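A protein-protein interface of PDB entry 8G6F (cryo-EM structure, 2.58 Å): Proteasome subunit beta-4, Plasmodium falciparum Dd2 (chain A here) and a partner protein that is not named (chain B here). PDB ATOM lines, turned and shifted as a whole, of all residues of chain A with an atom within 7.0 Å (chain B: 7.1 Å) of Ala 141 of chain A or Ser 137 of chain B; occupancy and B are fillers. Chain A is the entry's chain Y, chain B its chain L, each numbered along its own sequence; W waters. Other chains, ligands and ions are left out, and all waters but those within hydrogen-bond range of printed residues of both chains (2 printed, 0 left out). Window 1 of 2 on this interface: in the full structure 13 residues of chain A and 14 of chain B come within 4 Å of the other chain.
Of the printed residues of chain B, Ser 140 of chain A touches Arg 166.
Printed residues of chain B within 4 Å of Asp 144 of chain A: His 162 and Arg 166.
Tyr 147 of chain A touches none of the printed residues of chain B.
Of the printed residues of chain B, Glu 166 of chain A touches Tyr 136 (3.8 Å), Ser 137 (3.4 Å) and Asp 140 (3.0 Å).
Ala 135 of chain B touches none of the printed residues of chain A.
Of the printed residues of chain A, Tyr 136 of chain B touches Glu 166 and Arg 170.
Ser 137 of chain B touches just these residues of chain A: Leu 138 (2.9 Å), Ala 141 (3.3 Å), Ile 142 (3.8 Å) and Glu 166 (3.4 Å).
Of the printed residues of chain A, His 162 of chain B touches Asp 144 and Lys 145.
Water W1 lies within hydrogen-bond range of O of Tyr 137 of chain A (2.5 Å), N of Ala 141 of chain A (3.0 Å), OG of Ser 137 of chain B (3.1 Å), O of Leu 138 of chain A (3.4 Å) and N of Ser 140 of chain A (3.5 Å).
Water W2 bridges the backbone carbonyl oxygen (O) of His 162 of chain B (2.7 Å) and the side-chain carboxylate (OD2) of Asp 144 of chain A (3.1 Å).
Among the printed residues, pairs that only touch across the chains: Tyr 137 of chain A with Tyr 134 of chain B (3.3 Å), Leu 138 of chain A with Thr 133 of chain B (3.8 Å), Leu 138 of chain A with Ser 137 of chain B (2.9 Å), Ser 140 of chain A with Arg 166 of chain B (3.7 Å), Ala 141 of chain A with Tyr 134 of chain B (3.8 Å), Ala 141 of chain A with Ser 137 of chain B (3.3 Å), Ala 141 of chain A with Ile 138 of chain B (3.4 Å), Ile 142 of chain A with Ser 137 of chain B (3.8 Å), Ile 142 of chain A with Ser 141 of chain B (3.4 Å), Asp 144 of chain A with His 162 of chain B (3.9 Å), Lys 145 of chain A with Ile 138 of chain B (3.9 Å), Lys 145 of chain A with His 162 of chain B (3.4 Å), Tyr 146 of chain A with Ser 141 of chain B (3.7 Å), Glu 166 of chain A with Tyr 136 of chain B (3.8 Å), Glu 166 of chain A with Ser 137 of chain B (3.4 Å) and Arg 170 of chain A with Tyr 136 of chain B (3.5 Å).
Of the 15 printed residues of chain A, 10 touch a printed residue of chain B.
Hydrophobic or aromatic side chains of chain A that line the printed part of chain B: Tyr 137, Leu 138, Ala 141, Ile 142 and Tyr 146.
Of the 17 printed residues of chain B, 9 touch a printed residue of chain A.
Printed residues of chain B that touch a printed residue of chain A: Thr 133, Tyr 134, Tyr 136, Ser 137, Ile 138, Asp 140, Ser 141, His 162 and Arg 166.
Hydrophobic or aromatic side chains of chain B within 4 Å of the printed part of chain A: Tyr 134, Tyr 136, Ile 138 and His 162.
Among the printed residues, 20 pairs touch across the chains.
The backbone carbonyl oxygen of Ala 136 of chain A is in hydrogen-bond range of the side-chain hydroxyl of Ser 140 of chain A (2.8 Å).
The side-chain hydroxyl (OG) of Ser 137 of chain B lies within hydrogen-bond range of the backbone carbonyl oxygen (O) of Tyr 134 of chain B, 2.7 Å away.
The backbone carbonyl oxygen of Ser 137 of chain B sits at hydrogen-bond distance from the side-chain hydroxyl of Ser 141 of chain B (3.1 Å).
The side-chain hydroxyl of Thr 133 of chain B lies within hydrogen-bond range of the backbone carbonyl oxygen of Tyr 137 of chain A (3.4 Å).
The side-chain carboxylate (OD2) of Asp 144 of chain A is in salt-bridge range of the guanidinium group (NE) of Arg 166 of chain B (2.5 Å).
NH2 of Arg 170 of chain A is in salt-bridge range of OD1 of Asp 140 of chain B (2.8 Å).
OE2 of Glu 166 of chain A sits close to OD2 of Asp 140 of chain B, at 3.0 Å.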
ATOM      1  N   ALA A 136     -24.208 -28.414 -17.154  1.00  0.00           N
ATOM      2  CA  ALA A 136     -24.948 -28.001 -18.337  1.00  0.00           C
ATOM      3  C   ALA A 136     -24.379 -26.708 -18.899  1.00  0.00           C
ATOM      4  O   ALA A 136     -24.231 -26.563 -20.117  1.00  0.00           O
ATOM      5  CB  ALA A 136     -26.427 -27.836 -17.996  1.00  0.00           C
ATOM      6  N   TYR A 137     -24.025 -25.770 -18.020  1.00  0.00           N
ATOM      7  CA  TYR A 137     -23.449 -24.508 -18.464  1.00  0.00           C
ATOM      8  C   TYR A 137     -22.192 -24.719 -19.292  1.00  0.00           C
ATOM      9  O   TYR A 137     -21.882 -23.901 -20.162  1.00  0.00           O
ATOM     10  CB  TYR A 137     -23.131 -23.632 -17.256  1.00  0.00           C
ATOM     11  CG  TYR A 137     -24.349 -23.164 -16.503  1.00  0.00           C
ATOM     12  CD1 TYR A 137     -25.050 -22.043 -16.911  1.00  0.00           C
ATOM     13  CD2 TYR A 137     -24.798 -23.847 -15.384  1.00  0.00           C
ATOM     14  CE1 TYR A 137     -26.161 -21.614 -16.230  1.00  0.00           C
ATOM     15  CE2 TYR A 137     -25.910 -23.424 -14.694  1.00  0.00           C
ATOM     16  CZ  TYR A 137     -26.589 -22.308 -15.122  1.00  0.00           C
ATOM     17  OH  TYR A 137     -27.701 -21.878 -14.441  1.00  0.00           O
ATOM     18  N   LEU A 138     -21.457 -25.797 -19.044  1.00  0.00           N
ATOM     19  CA  LEU A 138     -20.191 -26.030 -19.719  1.00  0.00           C
ATOM     20  C   LEU A 138     -20.287 -27.005 -20.882  1.00  0.00           C
ATOM     21  O   LEU A 138     -19.357 -27.060 -21.691  1.00  0.00           O
ATOM     22  CB  LEU A 138     -19.152 -26.542 -18.720  1.00  0.00           C
ATOM     23  CG  LEU A 138     -18.720 -25.507 -17.688  1.00  0.00           C
ATOM     24  CD1 LEU A 138     -18.178 -26.185 -16.457  1.00  0.00           C
ATOM     25  CD2 LEU A 138     -17.696 -24.567 -18.288  1.00  0.00           C
ATOM     26  N   VAL A 139     -21.364 -27.778 -20.988  1.00  0.00           N
ATOM     27  CA  VAL A 139     -21.500 -28.731 -22.083  1.00  0.00           C
ATOM     28  C   VAL A 139     -22.546 -28.323 -23.119  1.00  0.00           C
ATOM     29  O   VAL A 139     -22.513 -28.850 -24.244  1.00  0.00           O
ATOM     30  CB  VAL A 139     -21.806 -30.146 -21.551  1.00  0.00           C
ATOM     31  CG1 VAL A 139     -20.760 -30.560 -20.537  1.00  0.00           C
ATOM     32  CG2 VAL A 139     -23.190 -30.208 -20.949  1.00  0.00           C
ATOM     33  N   SER A 140     -23.464 -27.409 -22.789  1.00  0.00           N
ATOM     34  CA  SER A 140     -24.547 -27.080 -23.710  1.00  0.00           C
ATOM     35  C   SER A 140     -24.023 -26.469 -24.998  1.00  0.00           C
ATOM     36  O   SER A 140     -24.495 -26.805 -26.089  1.00  0.00           O
ATOM     37  CB  SER A 140     -25.527 -26.128 -23.031  1.00  0.00           C
ATOM     38  OG  SER A 140     -26.230 -26.785 -21.997  1.00  0.00           O
ATOM     39  N   ALA A 141     -23.054 -25.560 -24.896  1.00  0.00           N
ATOM     40  CA  ALA A 141     -22.514 -24.923 -26.090  1.00  0.00           C
ATOM     41  C   ALA A 141     -21.713 -25.901 -26.936  1.00  0.00           C
ATOM     42  O   ALA A 141     -21.735 -25.805 -28.165  1.00  0.00           O
ATOM     43  CB  ALA A 141     -21.652 -23.726 -25.702  1.00  0.00           C
ATOM     44  N   ILE A 142     -20.999 -26.838 -26.311  1.00  0.00           N
ATOM     45  CA  ILE A 142     -20.297 -27.864 -27.079  1.00  0.00           C
ATOM     46  C   ILE A 142     -21.297 -28.690 -27.873  1.00  0.00           C
ATOM     47  O   ILE A 142     -21.100 -28.972 -29.063  1.00  0.00           O
ATOM     48  CB  ILE A 142     -19.453 -28.754 -26.148  1.00  0.00           C
ATOM     49  CG1 ILE A 142     -18.364 -27.940 -25.460  1.00  0.00           C
ATOM     50  CG2 ILE A 142     -18.828 -29.906 -26.928  1.00  0.00           C
ATOM     51  CD1 ILE A 142     -17.766 -28.629 -24.266  1.00  0.00           C
ATOM     52  N   LEU A 143     -22.387 -29.096 -27.218  1.00  0.00           N
ATOM     53  CA  LEU A 143     -23.433 -29.833 -27.917  1.00  0.00           C
ATOM     54  C   LEU A 143     -23.979 -29.024 -29.084  1.00  0.00           C
ATOM     55  O   LEU A 143     -24.086 -29.526 -30.208  1.00  0.00           O
ATOM     56  CB  LEU A 143     -24.555 -30.191 -26.946  1.00  0.00           C
ATOM     57  CG  LEU A 143     -24.215 -31.197 -25.849  1.00  0.00           C
ATOM     58  CD1 LEU A 143     -25.395 -31.383 -24.926  1.00  0.00           C
ATOM     59  CD2 LEU A 143     -23.794 -32.514 -26.454  1.00  0.00           C
ATOM     60  N   ASP A 144     -24.314 -27.756 -28.835  1.00  0.00           N
ATOM     61  CA  ASP A 144     -24.827 -26.891 -29.891  1.00  0.00           C
ATOM     62  C   ASP A 144     -23.866 -26.832 -31.069  1.00  0.00           C
ATOM     63  O   ASP A 144     -24.268 -26.989 -32.226  1.00  0.00           O
ATOM     64  CB  ASP A 144     -25.065 -25.484 -29.345  1.00  0.00           C
ATOM     65  CG  ASP A 144     -26.293 -25.392 -28.473  1.00  0.00           C
ATOM     66  OD1 ASP A 144     -27.178 -26.261 -28.585  1.00  0.00           O
ATOM     67  OD2 ASP A 144     -26.372 -24.444 -27.670  1.00  0.00           O
ATOM     68  N   LYS A 145     -22.585 -26.600 -30.788  1.00  0.00           N
ATOM     69  CA  LYS A 145     -21.615 -26.380 -31.852  1.00  0.00           C
ATOM     70  C   LYS A 145     -21.404 -27.635 -32.683  1.00  0.00           C
ATOM     71  O   LYS A 145     -21.438 -27.586 -33.916  1.00  0.00           O
ATOM     72  CB  LYS A 145     -20.289 -25.911 -31.262  1.00  0.00           C
ATOM     73  CG  LYS A 145     -19.332 -25.363 -32.292  1.00  0.00           C
ATOM     74  CD  LYS A 145     -17.949 -25.178 -31.726  1.00  0.00           C
ATOM     75  CE  LYS A 145     -16.915 -25.083 -32.825  1.00  0.00           C
ATOM     76  NZ  LYS A 145     -15.824 -24.143 -32.476  1.00  0.00           N
ATOM     77  N   TYR A 146     -21.166 -28.769 -32.030  1.00  0.00           N
ATOM     78  CA  TYR A 146     -20.738 -29.960 -32.751  1.00  0.00           C
ATOM     79  C   TYR A 146     -21.887 -30.869 -33.157  1.00  0.00           C
ATOM     80  O   TYR A 146     -21.650 -31.862 -33.850  1.00  0.00           O
ATOM     81  CB  TYR A 146     -19.729 -30.742 -31.911  1.00  0.00           C
ATOM     82  CG  TYR A 146     -18.441 -29.990 -31.699  1.00  0.00           C
ATOM     83  CD1 TYR A 146     -17.463 -29.965 -32.678  1.00  0.00           C
ATOM     84  CD2 TYR A 146     -18.207 -29.299 -30.523  1.00  0.00           C
ATOM     85  CE1 TYR A 146     -16.288 -29.278 -32.489  1.00  0.00           C
ATOM     86  CE2 TYR A 146     -17.036 -28.612 -30.326  1.00  0.00           C
ATOM     87  CZ  TYR A 146     -16.079 -28.604 -31.311  1.00  0.00           C
ATOM     88  OH  TYR A 146     -14.909 -27.916 -31.111  1.00  0.00           O
ATOM     89  N   TYR A 147     -23.116 -30.559 -32.764  1.00  0.00           N
ATOM     90  CA  TYR A 147     -24.260 -31.330 -33.217  1.00  0.00           C
ATOM     91  C   TYR A 147     -24.623 -30.954 -34.645  1.00  0.00           C
ATOM     92  O   TYR A 147     -24.575 -29.785 -35.028  1.00  0.00           O
ATOM     93  CB  TYR A 147     -25.456 -31.090 -32.300  1.00  0.00           C
ATOM     94  CG  TYR A 147     -26.706 -31.843 -32.692  1.00  0.00           C
ATOM     95  CD1 TYR A 147     -27.602 -31.313 -33.604  1.00  0.00           C
ATOM     96  CD2 TYR A 147     -26.998 -33.076 -32.133  1.00  0.00           C
ATOM     97  CE1 TYR A 147     -28.741 -31.994 -33.955  1.00  0.00           C
ATOM     98  CE2 TYR A 147     -28.136 -33.760 -32.479  1.00  0.00           C
ATOM     99  CZ  TYR A 147     -29.003 -33.215 -33.388  1.00  0.00           C
ATOM    100  OH  TYR A 147     -30.138 -33.900 -33.736  1.00  0.00           O
ATOM    101  N   LEU A 162     -15.614 -34.694 -25.837  1.00  0.00           N
ATOM    102  CA  LEU A 162     -15.336 -33.272 -25.663  1.00  0.00           C
ATOM    103  C   LEU A 162     -16.017 -32.734 -24.411  1.00  0.00           C
ATOM    104  O   LEU A 162     -15.413 -31.986 -23.633  1.00  0.00           O
ATOM    105  CB  LEU A 162     -15.806 -32.487 -26.886  1.00  0.00           C
ATOM    106  CG  LEU A 162     -15.015 -32.629 -28.181  1.00  0.00           C
ATOM    107  CD1 LEU A 162     -15.842 -32.108 -29.336  1.00  0.00           C
ATOM    108  CD2 LEU A 162     -13.693 -31.897 -28.091  1.00  0.00           C
ATOM    109  N   GLU A 166     -14.217 -31.182 -21.058  1.00  0.00           N
ATOM    110  CA  GLU A 166     -14.535 -29.856 -20.542  1.00  0.00           C
ATOM    111  C   GLU A 166     -14.942 -29.918 -19.075  1.00  0.00           C
ATOM    112  O   GLU A 166     -14.559 -29.055 -18.279  1.00  0.00           O
ATOM    113  CB  GLU A 166     -15.645 -29.223 -21.379  1.00  0.00           C
ATOM    114  CG  GLU A 166     -16.029 -27.823 -20.951  1.00  0.00           C
ATOM    115  CD  GLU A 166     -14.881 -26.851 -21.061  1.00  0.00           C
ATOM    116  OE1 GLU A 166     -13.871 -27.197 -21.703  1.00  0.00           O
ATOM    117  OE2 GLU A 166     -14.983 -25.741 -20.504  1.00  0.00           O
ATOM    118  N   ARG A 170     -12.601 -27.608 -16.687  1.00  0.00           N
ATOM    119  CA  ARG A 170     -13.081 -26.297 -16.287  1.00  0.00           C
ATOM    120  C   ARG A 170     -14.137 -26.325 -15.195  1.00  0.00           C
ATOM    121  O   ARG A 170     -14.336 -25.305 -14.534  1.00  0.00           O
ATOM    122  CB  ARG A 170     -13.646 -25.557 -17.509  1.00  0.00           C
ATOM    123  CG  ARG A 170     -13.884 -24.073 -17.313  1.00  0.00           C
ATOM    124  CD  ARG A 170     -12.597 -23.306 -17.116  1.00  0.00           C
ATOM    125  NE  ARG A 170     -11.822 -23.212 -18.344  1.00  0.00           N
ATOM    126  CZ  ARG A 170     -10.700 -22.519 -18.463  1.00  0.00           C
ATOM    127  NH1 ARG A 170     -10.192 -21.848 -17.446  1.00  0.00           N
ATOM    128  NH2 ARG A 170     -10.072 -22.499 -19.633  1.00  0.00           N
ATOM    129  N   GLY B 131     -22.496 -15.249 -20.037  1.00  0.00           N
ATOM    130  CA  GLY B 131     -22.190 -16.235 -21.051  1.00  0.00           C
ATOM    131  C   GLY B 131     -20.804 -16.824 -20.934  1.00  0.00           C
ATOM    132  O   GLY B 131     -20.363 -17.531 -21.851  1.00  0.00           O
ATOM    133  N   SER B 132     -20.106 -16.564 -19.829  1.00  0.00           N
ATOM    134  CA  SER B 132     -18.713 -16.965 -19.716  1.00  0.00           C
ATOM    135  C   SER B 132     -18.562 -18.475 -19.778  1.00  0.00           C
ATOM    136  O   SER B 132     -17.581 -18.975 -20.323  1.00  0.00           O
ATOM    137  CB  SER B 132     -18.114 -16.424 -18.422  1.00  0.00           C
ATOM    138  OG  SER B 132     -18.864 -16.832 -17.298  1.00  0.00           O
ATOM    139  N   THR B 133     -19.512 -19.220 -19.216  1.00  0.00           N
ATOM    140  CA  THR B 133     -19.397 -20.675 -19.231  1.00  0.00           C
ATOM    141  C   THR B 133     -19.472 -21.225 -20.650  1.00  0.00           C
ATOM    142  O   THR B 133     -18.677 -22.093 -21.031  1.00  0.00           O
ATOM    143  CB  THR B 133     -20.487 -21.292 -18.362  1.00  0.00           C
ATOM    144  OG1 THR B 133     -21.764 -20.772 -18.750  1.00  0.00           O
ATOM    145  CG2 THR B 133     -20.241 -20.975 -16.898  1.00  0.00           C
ATOM    146  N   TYR B 134     -20.418 -20.732 -21.449  1.00  0.00           N
ATOM    147  CA  TYR B 134     -20.527 -21.183 -22.830  1.00  0.00           C
ATOM    148  C   TYR B 134     -19.302 -20.782 -23.637  1.00  0.00           C
ATOM    149  O   TYR B 134     -18.765 -21.586 -24.414  1.00  0.00           O
ATOM    150  CB  TYR B 134     -21.795 -20.616 -23.459  1.00  0.00           C
ATOM    151  CG  TYR B 134     -23.023 -20.833 -22.618  1.00  0.00           C
ATOM    152  CD1 TYR B 134     -23.537 -22.105 -22.426  1.00  0.00           C
ATOM    153  CD2 TYR B 134     -23.665 -19.770 -22.005  1.00  0.00           C
ATOM    154  CE1 TYR B 134     -24.653 -22.311 -21.655  1.00  0.00           C
ATOM    155  CE2 TYR B 134     -24.783 -19.967 -21.232  1.00  0.00           C
ATOM    156  CZ  TYR B 134     -25.273 -21.239 -21.062  1.00  0.00           C
ATOM    157  OH  TYR B 134     -26.390 -21.442 -20.290  1.00  0.00           O
ATOM    158  N   ALA B 135     -18.840 -19.544 -23.460  1.00  0.00           N
ATOM    159  CA  ALA B 135     -17.631 -19.118 -24.152  1.00  0.00           C
ATOM    160  C   ALA B 135     -16.442 -19.973 -23.740  1.00  0.00           C
ATOM    161  O   ALA B 135     -15.613 -20.337 -24.577  1.00  0.00           O
ATOM    162  CB  ALA B 135     -17.362 -17.643 -23.871  1.00  0.00           C
ATOM    163  N   TYR B 136     -16.344 -20.301 -22.453  1.00  0.00           N
ATOM    164  CA  TYR B 136     -15.259 -21.139 -21.961  1.00  0.00           C
ATOM    165  C   TYR B 136     -15.290 -22.504 -22.616  1.00  0.00           C
ATOM    166  O   TYR B 136     -14.256 -23.028 -23.031  1.00  0.00           O
ATOM    167  CB  TYR B 136     -15.367 -21.299 -20.444  1.00  0.00           C
ATOM    168  CG  TYR B 136     -14.478 -20.398 -19.630  1.00  0.00           C
ATOM    169  CD1 TYR B 136     -13.129 -20.274 -19.914  1.00  0.00           C
ATOM    170  CD2 TYR B 136     -14.988 -19.689 -18.557  1.00  0.00           C
ATOM    171  CE1 TYR B 136     -12.321 -19.459 -19.166  1.00  0.00           C
ATOM    172  CE2 TYR B 136     -14.185 -18.874 -17.803  1.00  0.00           C
ATOM    173  CZ  TYR B 136     -12.852 -18.765 -18.110  1.00  0.00           C
ATOM    174  OH  TYR B 136     -12.048 -17.950 -17.356  1.00  0.00           O
ATOM    175  N   SER B 137     -16.469 -23.117 -22.682  1.00  0.00           N
ATOM    176  CA  SER B 137     -16.563 -24.443 -23.282  1.00  0.00           C
ATOM    177  C   SER B 137     -16.129 -24.405 -24.738  1.00  0.00           C
ATOM    178  O   SER B 137     -15.340 -25.247 -25.189  1.00  0.00           O
ATOM    179  CB  SER B 137     -17.986 -24.974 -23.154  1.00  0.00           C
ATOM    180  OG  SER B 137     -18.863 -24.285 -24.018  1.00  0.00           O
ATOM    181  N   ILE B 138     -16.614 -23.413 -25.487  1.00  0.00           N
ATOM    182  CA  ILE B 138     -16.263 -23.332 -26.902  1.00  0.00           C
ATOM    183  C   ILE B 138     -14.770 -23.089 -27.072  1.00  0.00           C
ATOM    184  O   ILE B 138     -14.125 -23.696 -27.932  1.00  0.00           O
ATOM    185  CB  ILE B 138     -17.098 -22.245 -27.603  1.00  0.00           C
ATOM    186  CG1 ILE B 138     -18.582 -22.599 -27.565  1.00  0.00           C
ATOM    187  CG2 ILE B 138     -16.640 -22.070 -29.037  1.00  0.00           C
ATOM    188  CD1 ILE B 138     -18.915 -23.939 -28.162  1.00  0.00           C
ATOM    189  N   LEU B 139     -14.198 -22.192 -26.268  1.00  0.00           N
ATOM    190  CA  LEU B 139     -12.773 -21.910 -26.381  1.00  0.00           C
ATOM    191  C   LEU B 139     -11.936 -23.123 -26.008  1.00  0.00           C
ATOM    192  O   LEU B 139     -10.954 -23.433 -26.683  1.00  0.00           O
ATOM    193  CB  LEU B 139     -12.400 -20.722 -25.499  1.00  0.00           C
ATOM    194  CG  LEU B 139     -12.929 -19.351 -25.920  1.00  0.00           C
ATOM    195  CD1 LEU B 139     -12.621 -18.326 -24.848  1.00  0.00           C
ATOM    196  CD2 LEU B 139     -12.350 -18.916 -27.254  1.00  0.00           C
ATOM    197  N   ASP B 140     -12.302 -23.823 -24.936  1.00  0.00           N
ATOM    198  CA  ASP B 140     -11.506 -24.954 -24.486  1.00  0.00           C
ATOM    199  C   ASP B 140     -11.572 -26.111 -25.467  1.00  0.00           C
ATOM    200  O   ASP B 140     -10.590 -26.844 -25.620  1.00  0.00           O
ATOM    201  CB  ASP B 140     -11.980 -25.414 -23.109  1.00  0.00           C
ATOM    202  CG  ASP B 140     -11.618 -24.437 -22.010  1.00  0.00           C
ATOM    203  OD1 ASP B 140     -10.498 -23.890 -22.038  1.00  0.00           O
ATOM    204  OD2 ASP B 140     -12.456 -24.219 -21.115  1.00  0.00           O
ATOM    205  N   SER B 141     -12.709 -26.300 -26.137  1.00  0.00           N
ATOM    206  CA  SER B 141     -12.823 -27.425 -27.054  1.00  0.00           C
ATOM    207  C   SER B 141     -11.988 -27.245 -28.314  1.00  0.00           C
ATOM    208  O   SER B 141     -11.720 -28.234 -29.001  1.00  0.00           O
ATOM    209  CB  SER B 141     -14.284 -27.642 -27.433  1.00  0.00           C
ATOM    210  OG  SER B 141     -15.031 -28.077 -26.314  1.00  0.00           O
ATOM    211  N   ALA B 142     -11.569 -26.017 -28.638  1.00  0.00           N
ATOM    212  CA  ALA B 142     -10.881 -25.780 -29.903  1.00  0.00           C
ATOM    213  C   ALA B 142      -9.719 -24.803 -29.782  1.00  0.00           C
ATOM    214  O   ALA B 142      -9.306 -24.225 -30.792  1.00  0.00           O
ATOM    215  CB  ALA B 142     -11.863 -25.257 -30.950  1.00  0.00           C
ATOM    216  N   TYR B 143      -9.173 -24.604 -28.591  1.00  0.00           N
ATOM    217  CA  TYR B 143      -8.095 -23.645 -28.416  1.00  0.00           C
ATOM    218  C   TYR B 143      -6.751 -24.262 -28.772  1.00  0.00           C
ATOM    219  O   TYR B 143      -6.503 -25.449 -28.550  1.00  0.00           O
ATOM    220  CB  TYR B 143      -8.055 -23.133 -26.978  1.00  0.00           C
ATOM    221  CG  TYR B 143      -6.889 -22.222 -26.694  1.00  0.00           C
ATOM    222  CD1 TYR B 143      -6.851 -20.936 -27.207  1.00  0.00           C
ATOM    223  CD2 TYR B 143      -5.827 -22.647 -25.914  1.00  0.00           C
ATOM    224  CE1 TYR B 143      -5.788 -20.100 -26.950  1.00  0.00           C
ATOM    225  CE2 TYR B 143      -4.760 -21.819 -25.651  1.00  0.00           C
ATOM    226  CZ  TYR B 143      -4.745 -20.547 -26.172  1.00  0.00           C
ATOM    227  OH  TYR B 143      -3.684 -19.721 -25.912  1.00  0.00           O
ATOM    228  N   ALA B 159     -17.211 -18.432 -30.338  1.00  0.00           N
ATOM    229  CA  ALA B 159     -17.483 -18.520 -28.909  1.00  0.00           C
ATOM    230  C   ALA B 159     -18.494 -17.466 -28.482  1.00  0.00           C
ATOM    231  O   ALA B 159     -19.437 -17.763 -27.735  1.00  0.00           O
ATOM    232  CB  ALA B 159     -16.185 -18.378 -28.120  1.00  0.00           C
ATOM    233  N   HIS B 162     -22.025 -18.478 -29.710  1.00  0.00           N
ATOM    234  CA  HIS B 162     -22.669 -19.533 -28.935  1.00  0.00           C
ATOM    235  C   HIS B 162     -23.093 -19.027 -27.564  1.00  0.00           C
ATOM    236  O   HIS B 162     -24.162 -19.399 -27.058  1.00  0.00           O
ATOM    237  CB  HIS B 162     -21.738 -20.734 -28.815  1.00  0.00           C
ATOM    238  CG  HIS B 162     -21.752 -21.613 -30.023  1.00  0.00           C
ATOM    239  ND1 HIS B 162     -22.829 -22.404 -30.354  1.00  0.00           N
ATOM    240  CD2 HIS B 162     -20.836 -21.799 -31.000  1.00  0.00           C
ATOM    241  CE1 HIS B 162     -22.570 -23.051 -31.473  1.00  0.00           C
ATOM    242  NE2 HIS B 162     -21.367 -22.701 -31.886  1.00  0.00           N
ATOM    243  N   ALA B 163     -22.276 -18.171 -26.949  1.00  0.00           N
ATOM    244  CA  ALA B 163     -22.672 -17.585 -25.676  1.00  0.00           C
ATOM    245  C   ALA B 163     -23.950 -16.769 -25.824  1.00  0.00           C
ATOM    246  O   ALA B 163     -24.860 -16.878 -24.997  1.00  0.00           O
ATOM    247  CB  ALA B 163     -21.542 -16.725 -25.122  1.00  0.00           C
ATOM    248  N   ARG B 166     -27.043 -19.169 -26.282  1.00  0.00           N
ATOM    249  CA  ARG B 166     -27.519 -19.904 -25.116  1.00  0.00           C
ATOM    250  C   ARG B 166     -27.903 -19.013 -23.943  1.00  0.00           C
ATOM    251  O   ARG B 166     -28.693 -19.441 -23.096  1.00  0.00           O
ATOM    252  CB  ARG B 166     -26.460 -20.903 -24.649  1.00  0.00           C
ATOM    253  CG  ARG B 166     -26.518 -22.230 -25.368  1.00  0.00           C
ATOM    254  CD  ARG B 166     -27.523 -23.165 -24.734  1.00  0.00           C
ATOM    255  NE  ARG B 166     -27.644 -24.407 -25.485  1.00  0.00           N
ATOM    256  CZ  ARG B 166     -28.510 -25.371 -25.209  1.00  0.00           C
ATOM    257  NH1 ARG B 166     -29.355 -25.273 -24.198  1.00  0.00           N
ATOM    258  NH2 ARG B 166     -28.526 -26.463 -25.964  1.00  0.00           N
HETATM  259  O   HOH W   1     -21.535 -24.537 -22.549  1.00  0.00           O
HETATM  260  O   HOH W   2     -25.044 -21.719 -28.068  1.00  0.00           O
